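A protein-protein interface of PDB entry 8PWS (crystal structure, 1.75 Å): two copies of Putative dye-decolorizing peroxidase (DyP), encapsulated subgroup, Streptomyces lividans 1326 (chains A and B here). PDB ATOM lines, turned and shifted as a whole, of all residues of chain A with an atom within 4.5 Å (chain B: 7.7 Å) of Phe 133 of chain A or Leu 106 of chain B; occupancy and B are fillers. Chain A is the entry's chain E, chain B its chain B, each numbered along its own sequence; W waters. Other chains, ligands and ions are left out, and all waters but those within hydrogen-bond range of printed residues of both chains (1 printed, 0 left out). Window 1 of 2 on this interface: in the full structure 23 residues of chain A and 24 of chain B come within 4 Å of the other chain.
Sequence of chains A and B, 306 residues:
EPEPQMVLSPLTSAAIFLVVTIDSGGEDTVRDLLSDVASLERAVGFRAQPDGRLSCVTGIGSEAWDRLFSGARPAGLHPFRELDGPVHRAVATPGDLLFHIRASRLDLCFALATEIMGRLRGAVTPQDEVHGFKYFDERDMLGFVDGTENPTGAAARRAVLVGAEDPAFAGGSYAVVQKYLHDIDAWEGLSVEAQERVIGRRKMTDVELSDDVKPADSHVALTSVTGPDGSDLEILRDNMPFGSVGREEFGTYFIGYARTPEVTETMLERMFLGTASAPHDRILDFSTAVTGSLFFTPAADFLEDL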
ATOM      1  N   SER A  13     -21.706  19.420 -17.964  1.00  0.00           N
ATOM      2  CA  SER A  13     -21.545  20.530 -17.043  1.00  0.00           C
ATOM      3  C   SER A  13     -20.322  20.369 -16.121  1.00  0.00           C
ATOM      4  O   SER A  13     -20.002  21.259 -15.372  1.00  0.00           O
ATOM      5  CB  SER A  13     -22.832  20.688 -16.288  1.00  0.00           C
ATOM      6  OG  SER A  13     -23.227  19.412 -15.885  1.00  0.00           O
ATOM      7  N   LEU A 106     -19.271  15.858 -11.520  1.00  0.00           N
ATOM      8  CA  LEU A 106     -17.839  15.824 -11.301  1.00  0.00           C
ATOM      9  C   LEU A 106     -17.342  14.459 -10.797  1.00  0.00           C
ATOM     10  O   LEU A 106     -16.239  14.023 -11.155  1.00  0.00           O
ATOM     11  CB  LEU A 106     -17.471  16.935 -10.335  1.00  0.00           C
ATOM     12  CG  LEU A 106     -15.970  17.147 -10.190  1.00  0.00           C
ATOM     13  CD1 LEU A 106     -15.336  17.483 -11.539  1.00  0.00           C
ATOM     14  CD2 LEU A 106     -15.673  18.259  -9.204  1.00  0.00           C
ATOM     15  N   HIS A 131     -10.395  21.059 -12.402  1.00  0.00           N
ATOM     16  CA  HIS A 131     -11.746  20.577 -12.199  1.00  0.00           C
ATOM     17  C   HIS A 131     -12.664  21.696 -12.624  1.00  0.00           C
ATOM     18  O   HIS A 131     -12.671  22.716 -11.966  1.00  0.00           O
ATOM     19  CB  HIS A 131     -12.010  20.185 -10.730  1.00  0.00           C
ATOM     20  CG  HIS A 131     -11.152  19.072 -10.224  1.00  0.00           C
ATOM     21  ND1 HIS A 131     -11.322  18.510  -8.985  1.00  0.00           N
ATOM     22  CD2 HIS A 131     -10.141  18.378 -10.807  1.00  0.00           C
ATOM     23  CE1 HIS A 131     -10.397  17.573  -8.792  1.00  0.00           C
ATOM     24  NE2 HIS A 131      -9.674  17.463  -9.902  1.00  0.00           N
ATOM     25  N   GLY A 132     -13.362  21.505 -13.737  1.00  0.00           N
ATOM     26  CA  GLY A 132     -14.137  22.564 -14.350  1.00  0.00           C
ATOM     27  C   GLY A 132     -15.624  22.375 -14.096  1.00  0.00           C
ATOM     28  O   GLY A 132     -16.082  21.241 -13.962  1.00  0.00           O
ATOM     29  N   PHE A 133     -16.372  23.483 -14.058  1.00  0.00           N
ATOM     30  CA  PHE A 133     -17.815  23.458 -13.826  1.00  0.00           C
ATOM     31  C   PHE A 133     -18.484  24.537 -14.678  1.00  0.00           C
ATOM     32  O   PHE A 133     -18.060  25.664 -14.707  1.00  0.00           O
ATOM     33  CB  PHE A 133     -18.144  23.669 -12.345  1.00  0.00           C
ATOM     34  CG  PHE A 133     -17.415  24.824 -11.683  1.00  0.00           C
ATOM     35  CD1 PHE A 133     -17.895  26.138 -11.743  1.00  0.00           C
ATOM     36  CD2 PHE A 133     -16.228  24.600 -10.988  1.00  0.00           C
ATOM     37  CE1 PHE A 133     -17.197  27.198 -11.170  1.00  0.00           C
ATOM     38  CE2 PHE A 133     -15.559  25.662 -10.375  1.00  0.00           C
ATOM     39  CZ  PHE A 133     -16.052  26.960 -10.470  1.00  0.00           C
ATOM     40  N   LYS A 134     -19.534  24.210 -15.390  1.00  0.00           N
ATOM     41  CA  LYS A 134     -20.217  25.204 -16.194  1.00  0.00           C
ATOM     42  C   LYS A 134     -21.242  25.892 -15.302  1.00  0.00           C
ATOM     43  O   LYS A 134     -21.776  25.286 -14.402  1.00  0.00           O
ATOM     44  CB  LYS A 134     -20.827  24.556 -17.440  1.00  0.00           C
ATOM     45  CG  LYS A 134     -20.998  25.495 -18.633  1.00  0.00           C
ATOM     46  CD  LYS A 134     -19.685  25.836 -19.373  1.00  0.00           C
ATOM     47  CE  LYS A 134     -19.744  27.088 -20.242  1.00  0.00           C
ATOM     48  NZ  LYS A 134     -20.298  26.740 -21.569  1.00  0.00           N
ATOM     49  N   TYR A 135     -21.460  27.187 -15.501  1.00  0.00           N
ATOM     50  CA  TYR A 135     -22.566  27.904 -14.865  1.00  0.00           C
ATOM     51  C   TYR A 135     -23.916  27.513 -15.470  1.00  0.00           C
ATOM     52  O   TYR A 135     -23.993  26.922 -16.549  1.00  0.00           O
ATOM     53  CB  TYR A 135     -22.406  29.411 -14.992  1.00  0.00           C
ATOM     54  CG  TYR A 135     -21.366  29.911 -14.017  1.00  0.00           C
ATOM     55  CD1 TYR A 135     -20.054  29.868 -14.368  1.00  0.00           C
ATOM     56  CD2 TYR A 135     -21.670  30.298 -12.729  1.00  0.00           C
ATOM     57  CE1 TYR A 135     -19.063  30.316 -13.516  1.00  0.00           C
ATOM     58  CE2 TYR A 135     -20.698  30.734 -11.862  1.00  0.00           C
ATOM     59  CZ  TYR A 135     -19.390  30.725 -12.252  1.00  0.00           C
ATOM     60  OH  TYR A 135     -18.378  31.074 -11.448  1.00  0.00           O
ATOM     61  N   MET A 240     -14.254  25.845 -19.988  1.00  0.00           N
ATOM     62  CA  MET A 240     -14.800  25.512 -18.682  1.00  0.00           C
ATOM     63  C   MET A 240     -14.255  26.482 -17.669  1.00  0.00           C
ATOM     64  O   MET A 240     -13.056  26.673 -17.579  1.00  0.00           O
ATOM     65  CB  MET A 240     -14.392  24.105 -18.227  1.00  0.00           C
ATOM     66  CG  MET A 240     -15.080  23.002 -19.001  1.00  0.00           C
ATOM     67  SD  MET A 240     -16.894  22.994 -18.987  1.00  0.00           S
ATOM     68  CE  MET A 240     -17.156  22.354 -17.363  1.00  0.00           C
ATOM     69  N   PRO A 241     -15.127  27.112 -16.862  1.00  0.00           N
ATOM     70  CA  PRO A 241     -14.687  27.845 -15.684  1.00  0.00           C
ATOM     71  C   PRO A 241     -14.065  26.911 -14.650  1.00  0.00           C
ATOM     72  O   PRO A 241     -14.389  25.735 -14.541  1.00  0.00           O
ATOM     73  CB  PRO A 241     -15.986  28.374 -15.086  1.00  0.00           C
ATOM     74  CG  PRO A 241     -16.949  28.369 -16.250  1.00  0.00           C
ATOM     75  CD  PRO A 241     -16.577  27.171 -17.083  1.00  0.00           C
ATOM     76  N   PHE A 242     -13.181  27.482 -13.859  1.00  0.00           N
ATOM     77  CA  PHE A 242     -12.598  26.813 -12.713  1.00  0.00           C
ATOM     78  C   PHE A 242     -12.143  27.894 -11.743  1.00  0.00           C
ATOM     79  O   PHE A 242     -12.030  29.047 -12.107  1.00  0.00           O
ATOM     80  CB  PHE A 242     -11.408  25.925 -13.101  1.00  0.00           C
ATOM     81  CG  PHE A 242     -10.185  26.680 -13.528  1.00  0.00           C
ATOM     82  CD1 PHE A 242     -10.039  27.069 -14.853  1.00  0.00           C
ATOM     83  CD2 PHE A 242      -9.216  27.023 -12.618  1.00  0.00           C
ATOM     84  CE1 PHE A 242      -8.912  27.777 -15.262  1.00  0.00           C
ATOM     85  CE2 PHE A 242      -8.090  27.716 -13.011  1.00  0.00           C
ATOM     86  CZ  PHE A 242      -7.955  28.117 -14.328  1.00  0.00           C
ATOM     87  N   GLY A 243     -11.874  27.489 -10.509  1.00  0.00           N
ATOM     88  CA  GLY A 243     -11.236  28.382  -9.608  1.00  0.00           C
ATOM     89  C   GLY A 243     -11.184  27.902  -8.163  1.00  0.00           C
ATOM     90  O   GLY A 243     -11.638  26.831  -7.781  1.00  0.00           O
ATOM     91  N   SER B  13     -25.645  17.130  -4.087  1.00  0.00           N
ATOM     92  CA  SER B  13     -24.535  16.341  -4.605  1.00  0.00           C
ATOM     93  C   SER B  13     -23.263  17.181  -4.723  1.00  0.00           C
ATOM     94  O   SER B  13     -22.238  16.625  -5.061  1.00  0.00           O
ATOM     95  CB  SER B  13     -24.948  15.718  -5.910  1.00  0.00           C
ATOM     96  OG  SER B  13     -25.608  16.725  -6.637  1.00  0.00           O
ATOM     97  N   ALA B  14     -23.302  18.480  -4.367  1.00  0.00           N
ATOM     98  CA  ALA B  14     -22.105  19.304  -4.358  1.00  0.00           C
ATOM     99  C   ALA B  14     -22.058  20.147  -3.098  1.00  0.00           C
ATOM    100  O   ALA B  14     -23.107  20.526  -2.571  1.00  0.00           O
ATOM    101  CB  ALA B  14     -22.086  20.193  -5.569  1.00  0.00           C
ATOM    102  N   ALA B  15     -20.842  20.479  -2.671  1.00  0.00           N
ATOM    103  CA  ALA B  15     -20.660  21.328  -1.512  1.00  0.00           C
ATOM    104  C   ALA B  15     -19.346  22.089  -1.609  1.00  0.00           C
ATOM    105  O   ALA B  15     -18.387  21.623  -2.204  1.00  0.00           O
ATOM    106  CB  ALA B  15     -20.727  20.551  -0.225  1.00  0.00           C
ATOM    107  N   ILE B  16     -19.340  23.274  -1.010  1.00  0.00           N
ATOM    108  CA  ILE B  16     -18.123  23.978  -0.669  1.00  0.00           C
ATOM    109  C   ILE B  16     -18.092  24.188   0.836  1.00  0.00           C
ATOM    110  O   ILE B  16     -19.056  24.658   1.420  1.00  0.00           O
ATOM    111  CB  ILE B  16     -17.960  25.278  -1.456  1.00  0.00           C
ATOM    112  CG1 ILE B  16     -17.692  24.979  -2.946  1.00  0.00           C
ATOM    113  CG2 ILE B  16     -16.826  26.104  -0.846  1.00  0.00           C
ATOM    114  CD1 ILE B  16     -17.479  26.196  -3.835  1.00  0.00           C
ATOM    115  N   LEU B  54     -29.776  25.393  -3.494  1.00  0.00           N
ATOM    116  CA  LEU B  54     -28.658  26.090  -2.873  1.00  0.00           C
ATOM    117  C   LEU B  54     -28.994  26.497  -1.448  1.00  0.00           C
ATOM    118  O   LEU B  54     -30.014  27.079  -1.229  1.00  0.00           O
ATOM    119  CB  LEU B  54     -28.322  27.331  -3.692  1.00  0.00           C
ATOM    120  CG  LEU B  54     -27.209  28.186  -3.117  1.00  0.00           C
ATOM    121  CD1 LEU B  54     -25.855  27.490  -3.154  1.00  0.00           C
ATOM    122  CD2 LEU B  54     -27.130  29.478  -3.872  1.00  0.00           C
ATOM    123  N   ILE B 101     -21.748  25.345   2.260  1.00  0.00           N
ATOM    124  CA  ILE B 101     -22.544  25.697   1.117  1.00  0.00           C
ATOM    125  C   ILE B 101     -22.867  24.432   0.334  1.00  0.00           C
ATOM    126  O   ILE B 101     -21.948  23.686  -0.003  1.00  0.00           O
ATOM    127  CB  ILE B 101     -21.789  26.720   0.263  1.00  0.00           C
ATOM    128  CG1 ILE B 101     -21.385  27.944   1.107  1.00  0.00           C
ATOM    129  CG2 ILE B 101     -22.628  27.098  -0.940  1.00  0.00           C
ATOM    130  CD1 ILE B 101     -20.355  28.868   0.460  1.00  0.00           C
ATOM    131  N   ARG B 102     -24.164  24.195   0.069  1.00  0.00           N
ATOM    132  CA  ARG B 102     -24.614  22.998  -0.612  1.00  0.00           C
ATOM    133  C   ARG B 102     -25.513  23.360  -1.772  1.00  0.00           C
ATOM    134  O   ARG B 102     -26.312  24.271  -1.678  1.00  0.00           O
ATOM    135  CB  ARG B 102     -25.373  22.088   0.347  1.00  0.00           C
ATOM    136  CG  ARG B 102     -24.467  21.401   1.364  1.00  0.00           C
ATOM    137  CD  ARG B 102     -25.222  20.567   2.370  1.00  0.00           C
ATOM    138  NE  ARG B 102     -25.890  21.367   3.361  1.00  0.00           N
ATOM    139  CZ  ARG B 102     -26.447  20.877   4.467  1.00  0.00           C
ATOM    140  NH1 ARG B 102     -26.374  19.583   4.706  1.00  0.00           N
ATOM    141  NH2 ARG B 102     -27.028  21.662   5.356  1.00  0.00           N
ATOM    142  N   ALA B 103     -25.444  22.540  -2.814  1.00  0.00           N
ATOM    143  CA  ALA B 103     -26.392  22.637  -3.907  1.00  0.00           C
ATOM    144  C   ALA B 103     -26.379  21.369  -4.757  1.00  0.00           C
ATOM    145  O   ALA B 103     -25.593  20.460  -4.527  1.00  0.00           O
ATOM    146  CB  ALA B 103     -26.038  23.841  -4.736  1.00  0.00           C
ATOM    147  N   SER B 104     -27.227  21.350  -5.786  1.00  0.00           N
ATOM    148  CA  SER B 104     -27.224  20.243  -6.717  1.00  0.00           C
ATOM    149  C   SER B 104     -26.090  20.380  -7.726  1.00  0.00           C
ATOM    150  O   SER B 104     -25.823  19.440  -8.434  1.00  0.00           O
ATOM    151  CB  SER B 104     -28.534  20.136  -7.392  1.00  0.00           C
ATOM    152  OG  SER B 104     -28.721  21.260  -8.238  1.00  0.00           O
ATOM    153  N   ARG B 105     -25.388  21.512  -7.780  1.00  0.00           N
ATOM    154  CA  ARG B 105     -24.313  21.708  -8.751  1.00  0.00           C
ATOM    155  C   ARG B 105     -23.248  22.619  -8.155  1.00  0.00           C
ATOM    156  O   ARG B 105     -23.572  23.559  -7.449  1.00  0.00           O
ATOM    157  CB  ARG B 105     -24.765  22.563  -9.946  1.00  0.00           C
ATOM    158  CG  ARG B 105     -26.057  22.203 -10.645  1.00  0.00           C
ATOM    159  CD  ARG B 105     -26.523  23.319 -11.590  1.00  0.00           C
ATOM    160  NE  ARG B 105     -25.512  23.710 -12.568  1.00  0.00           N
ATOM    161  CZ  ARG B 105     -25.419  23.341 -13.841  1.00  0.00           C
ATOM    162  NH1 ARG B 105     -26.288  22.509 -14.371  1.00  0.00           N
ATOM    163  NH2 ARG B 105     -24.438  23.811 -14.602  1.00  0.00           N
ATOM    164  N   LEU B 106     -21.983  22.347  -8.465  1.00  0.00           N
ATOM    165  CA  LEU B 106     -20.883  23.052  -7.852  1.00  0.00           C
ATOM    166  C   LEU B 106     -20.828  24.538  -8.217  1.00  0.00           C
ATOM    167  O   LEU B 106     -20.439  25.342  -7.388  1.00  0.00           O
ATOM    168  CB  LEU B 106     -19.607  22.327  -8.266  1.00  0.00           C
ATOM    169  CG  LEU B 106     -18.359  22.800  -7.577  1.00  0.00           C
ATOM    170  CD1 LEU B 106     -18.482  22.599  -6.066  1.00  0.00           C
ATOM    171  CD2 LEU B 106     -17.180  22.017  -8.150  1.00  0.00           C
ATOM    172  N   ASP B 107     -21.266  24.913  -9.427  1.00  0.00           N
ATOM    173  CA  ASP B 107     -21.229  26.300  -9.868  1.00  0.00           C
ATOM    174  C   ASP B 107     -22.027  27.210  -8.954  1.00  0.00           C
ATOM    175  O   ASP B 107     -21.619  28.325  -8.698  1.00  0.00           O
ATOM    176  CB  ASP B 107     -21.731  26.500 -11.309  1.00  0.00           C
ATOM    177  CG  ASP B 107     -23.084  25.895 -11.623  1.00  0.00           C
ATOM    178  OD1 ASP B 107     -23.059  24.636 -11.642  1.00  0.00           O
ATOM    179  OD2 ASP B 107     -24.123  26.667 -11.850  1.00  0.00           O
ATOM    180  N   LEU B 108     -23.195  26.782  -8.493  1.00  0.00           N
ATOM    181  CA  LEU B 108     -23.989  27.600  -7.581  1.00  0.00           C
ATOM    182  C   LEU B 108     -23.267  27.757  -6.260  1.00  0.00           C
ATOM    183  O   LEU B 108     -23.339  28.833  -5.676  1.00  0.00           O
ATOM    184  CB  LEU B 108     -25.343  26.921  -7.315  1.00  0.00           C
ATOM    185  CG  LEU B 108     -26.307  26.948  -8.476  1.00  0.00           C
ATOM    186  CD1 LEU B 108     -27.525  26.159  -8.109  1.00  0.00           C
ATOM    187  CD2 LEU B 108     -26.703  28.389  -8.787  1.00  0.00           C
ATOM    188  N   CYS B 109     -22.640  26.674  -5.778  1.00  0.00           N
ATOM    189  CA  CYS B 109     -21.867  26.778  -4.558  1.00  0.00           C
ATOM    190  C   CYS B 109     -20.769  27.815  -4.734  1.00  0.00           C
ATOM    191  O   CYS B 109     -20.550  28.672  -3.858  1.00  0.00           O
ATOM    192  CB  CYS B 109     -21.237  25.452  -4.178  1.00  0.00           C
ATOM    193  SG  CYS B 109     -22.437  24.162  -3.785  1.00  0.00           S
ATOM    194  N   PHE B 110     -20.081  27.746  -5.878  1.00  0.00           N
ATOM    195  CA  PHE B 110     -18.960  28.635  -6.138  1.00  0.00           C
ATOM    196  C   PHE B 110     -19.434  30.084  -6.246  1.00  0.00           C
ATOM    197  O   PHE B 110     -18.775  30.991  -5.765  1.00  0.00           O
ATOM    198  CB  PHE B 110     -18.242  28.176  -7.402  1.00  0.00           C
ATOM    199  CG  PHE B 110     -16.898  28.823  -7.598  1.00  0.00           C
ATOM    200  CD1 PHE B 110     -15.755  28.315  -6.996  1.00  0.00           C
ATOM    201  CD2 PHE B 110     -16.802  29.933  -8.403  1.00  0.00           C
ATOM    202  CE1 PHE B 110     -14.543  28.958  -7.155  1.00  0.00           C
ATOM    203  CE2 PHE B 110     -15.564  30.537  -8.617  1.00  0.00           C
ATOM    204  CZ  PHE B 110     -14.452  30.079  -7.969  1.00  0.00           C
ATOM    205  N   ALA B 111     -20.573  30.311  -6.905  1.00  0.00           N
ATOM    206  CA  ALA B 111     -21.091  31.649  -7.087  1.00  0.00           C
ATOM    207  C   ALA B 111     -21.377  32.299  -5.746  1.00  0.00           C
ATOM    208  O   ALA B 111     -21.008  33.443  -5.511  1.00  0.00           O
ATOM    209  CB  ALA B 111     -22.303  31.585  -7.970  1.00  0.00           C
ATOM    210  N   LEU B 112     -21.994  31.542  -4.832  1.00  0.00           N
ATOM    211  CA  LEU B 112     -22.267  32.089  -3.501  1.00  0.00           C
ATOM    212  C   LEU B 112     -20.971  32.290  -2.712  1.00  0.00           C
ATOM    213  O   LEU B 112     -20.803  33.304  -2.052  1.00  0.00           O
ATOM    214  CB  LEU B 112     -23.271  31.198  -2.760  1.00  0.00           C
ATOM    215  CG  LEU B 112     -23.596  31.671  -1.330  1.00  0.00           C
ATOM    216  CD1 LEU B 112     -24.200  33.069  -1.304  1.00  0.00           C
ATOM    217  CD2 LEU B 112     -24.543  30.739  -0.613  1.00  0.00           C
ATOM    218  N   ALA B 113     -20.047  31.316  -2.746  1.00  0.00           N
ATOM    219  CA  ALA B 113     -18.766  31.474  -2.066  1.00  0.00           C
ATOM    220  C   ALA B 113     -18.026  32.723  -2.552  1.00  0.00           C
ATOM    221  O   ALA B 113     -17.417  33.420  -1.756  1.00  0.00           O
ATOM    222  CB  ALA B 113     -17.883  30.248  -2.244  1.00  0.00           C
ATOM    223  N   THR B 114     -18.070  32.981  -3.862  1.00  0.00           N
ATOM    224  CA  THR B 114     -17.436  34.150  -4.439  1.00  0.00           C
ATOM    225  C   THR B 114     -18.029  35.423  -3.830  1.00  0.00           C
ATOM    226  O   THR B 114     -17.278  36.328  -3.483  1.00  0.00           O
ATOM    227  CB  THR B 114     -17.592  34.159  -5.969  1.00  0.00           C
ATOM    228  OG1 THR B 114     -16.870  33.048  -6.472  1.00  0.00           O
ATOM    229  CG2 THR B 114     -17.021  35.404  -6.606  1.00  0.00           C
ATOM    230  N   VAL B 130     -12.739  23.359   0.559  1.00  0.00           N
ATOM    231  CA  VAL B 130     -12.879  22.040   0.004  1.00  0.00           C
ATOM    232  C   VAL B 130     -14.106  22.041  -0.904  1.00  0.00           C
ATOM    233  O   VAL B 130     -15.177  22.530  -0.530  1.00  0.00           O
ATOM    234  CB  VAL B 130     -13.014  20.980   1.109  1.00  0.00           C
ATOM    235  CG1 VAL B 130     -13.420  19.624   0.553  1.00  0.00           C
ATOM    236  CG2 VAL B 130     -11.746  20.843   1.888  1.00  0.00           C
ATOM    237  N   HIS B 131     -13.928  21.466  -2.103  1.00  0.00           N
ATOM    238  CA  HIS B 131     -14.973  21.351  -3.102  1.00  0.00           C
ATOM    239  C   HIS B 131     -15.349  19.889  -3.112  1.00  0.00           C
ATOM    240  O   HIS B 131     -14.519  19.072  -3.460  1.00  0.00           O
ATOM    241  CB  HIS B 131     -14.528  21.807  -4.501  1.00  0.00           C
ATOM    242  CG  HIS B 131     -14.107  23.251  -4.567  1.00  0.00           C
ATOM    243  ND1 HIS B 131     -13.854  23.881  -5.770  1.00  0.00           N
ATOM    244  CD2 HIS B 131     -13.969  24.202  -3.605  1.00  0.00           C
ATOM    245  CE1 HIS B 131     -13.520  25.150  -5.522  1.00  0.00           C
ATOM    246  NE2 HIS B 131     -13.562  25.356  -4.211  1.00  0.00           N
ATOM    247  N   GLY B 132     -16.550  19.600  -2.603  1.00  0.00           N
ATOM    248  CA  GLY B 132     -16.987  18.236  -2.412  1.00  0.00           C
ATOM    249  C   GLY B 132     -17.948  17.800  -3.490  1.00  0.00           C
ATOM    250  O   GLY B 132     -18.703  18.616  -4.021  1.00  0.00           O
ATOM    251  N   PHE B 133     -17.965  16.494  -3.766  1.00  0.00           N
ATOM    252  CA  PHE B 133     -18.855  15.903  -4.758  1.00  0.00           C
ATOM    253  C   PHE B 133     -19.349  14.542  -4.266  1.00  0.00           C
ATOM    254  O   PHE B 133     -18.567  13.739  -3.855  1.00  0.00           O
ATOM    255  CB  PHE B 133     -18.159  15.756  -6.105  1.00  0.00           C
ATOM    256  CG  PHE B 133     -16.761  15.167  -6.068  1.00  0.00           C
ATOM    257  CD1 PHE B 133     -16.562  13.795  -6.103  1.00  0.00           C
ATOM    258  CD2 PHE B 133     -15.648  15.987  -5.991  1.00  0.00           C
ATOM    259  CE1 PHE B 133     -15.282  13.252  -6.048  1.00  0.00           C
ATOM    260  CE2 PHE B 133     -14.373  15.449  -5.959  1.00  0.00           C
ATOM    261  CZ  PHE B 133     -14.193  14.078  -5.990  1.00  0.00           C
HETATM  262  O   HOH W   1     -24.821  24.232 -17.716  1.00  0.00           O
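The backbone carbonyl oxygen (O) of Lys 134 of chain A sits close to the side-chain carboxylate (OD1) of Asp 107 of chain B.
The guanidinium group of Arg 105 of chain B lies within hydrogen-bond range of the backbone carbonyl oxygen of Lys 134 of chain A.
The backbone carbonyl oxygen of Ser 13 of chain A is in hydrogen-bond range of the backbone NH of Lys 134 of chain A (3.0 Å).
The backbone NH (N) of Phe 133 of chain A sits at hydrogen-bond distance from the backbone carbonyl oxygen (O) of Pro 241 of chain A (3.0 Å).
The backbone carbonyl oxygen of Phe 110 of chain B sits at hydrogen-bond distance from the side-chain hydroxyl of Thr 114 of chain B.
NE of Arg 105 of chain B lies within salt-bridge range of OD1 of Asp 107 of chain B.
Among the printed residues, pairs that only touch across the chains: Ser 13 of chain A with Arg 105 of chain B, Leu 106 of chain A with Phe 133 of chain B, Phe 133 of chain A with Leu 106 of chain B, Phe 133 of chain A with Asp 107 of chain B, Phe 133 of chain A with Phe 110 of chain B, Tyr 135 of chain A with Arg 105 of chain B, Tyr 135 of chain A with Asp 107 of chain B, Tyr 135 of chain A with Phe 110 of chain B, Gly 243 of chain A with Phe 110 of chain B and Gly 243 of chain A with His 131 of chain B.
Printed residues of chain B within 4 Å of Leu 106 of chain A: Phe 133 (3.9 Å).
Of the printed residues of chain B, Gly 243 of chain A touches Phe 110 and His 131.
Printed residues of chain A within 4 Å of Asp 107 of chain B: Phe 133 (3.8 Å), Lys 134 (3.1 Å) and Tyr 135 (3.6 Å).
The nearest residue of chain B that does not touch Phe 133 of chain A is His 131 of chain B (5.2 Å).
The nearest residue of chain A that does not touch Leu 106 of chain B is Leu 106 of chain A (4.2 Å).
Of the 11 printed residues of chain A, 6 touch a printed residue of chain B.
Hydrophobic or aromatic side chains of chain A within 4 Å of the printed part of chain B: Leu 106, Phe 133 and Tyr 135.
Printed residues of chain B that touch a printed residue of chain A: Arg 105, Leu 106, Asp 107, Phe 110, His 131 and Phe 133.
Hydrophobic or aromatic side chains of chain B that line the printed part of chain A: Leu 106, Phe 110, His 131 and Phe 133.
Leu 106 of chain A touches Phe 133 of chain B, and with the chains exchanged Phe 133 of chain A touches Leu 106 of chain B.
Water W1 lies within hydrogen-bond range of O of Tyr 135 of chain A (3.0 Å) and NH2 of Arg 105 of chain B (3.2 Å).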
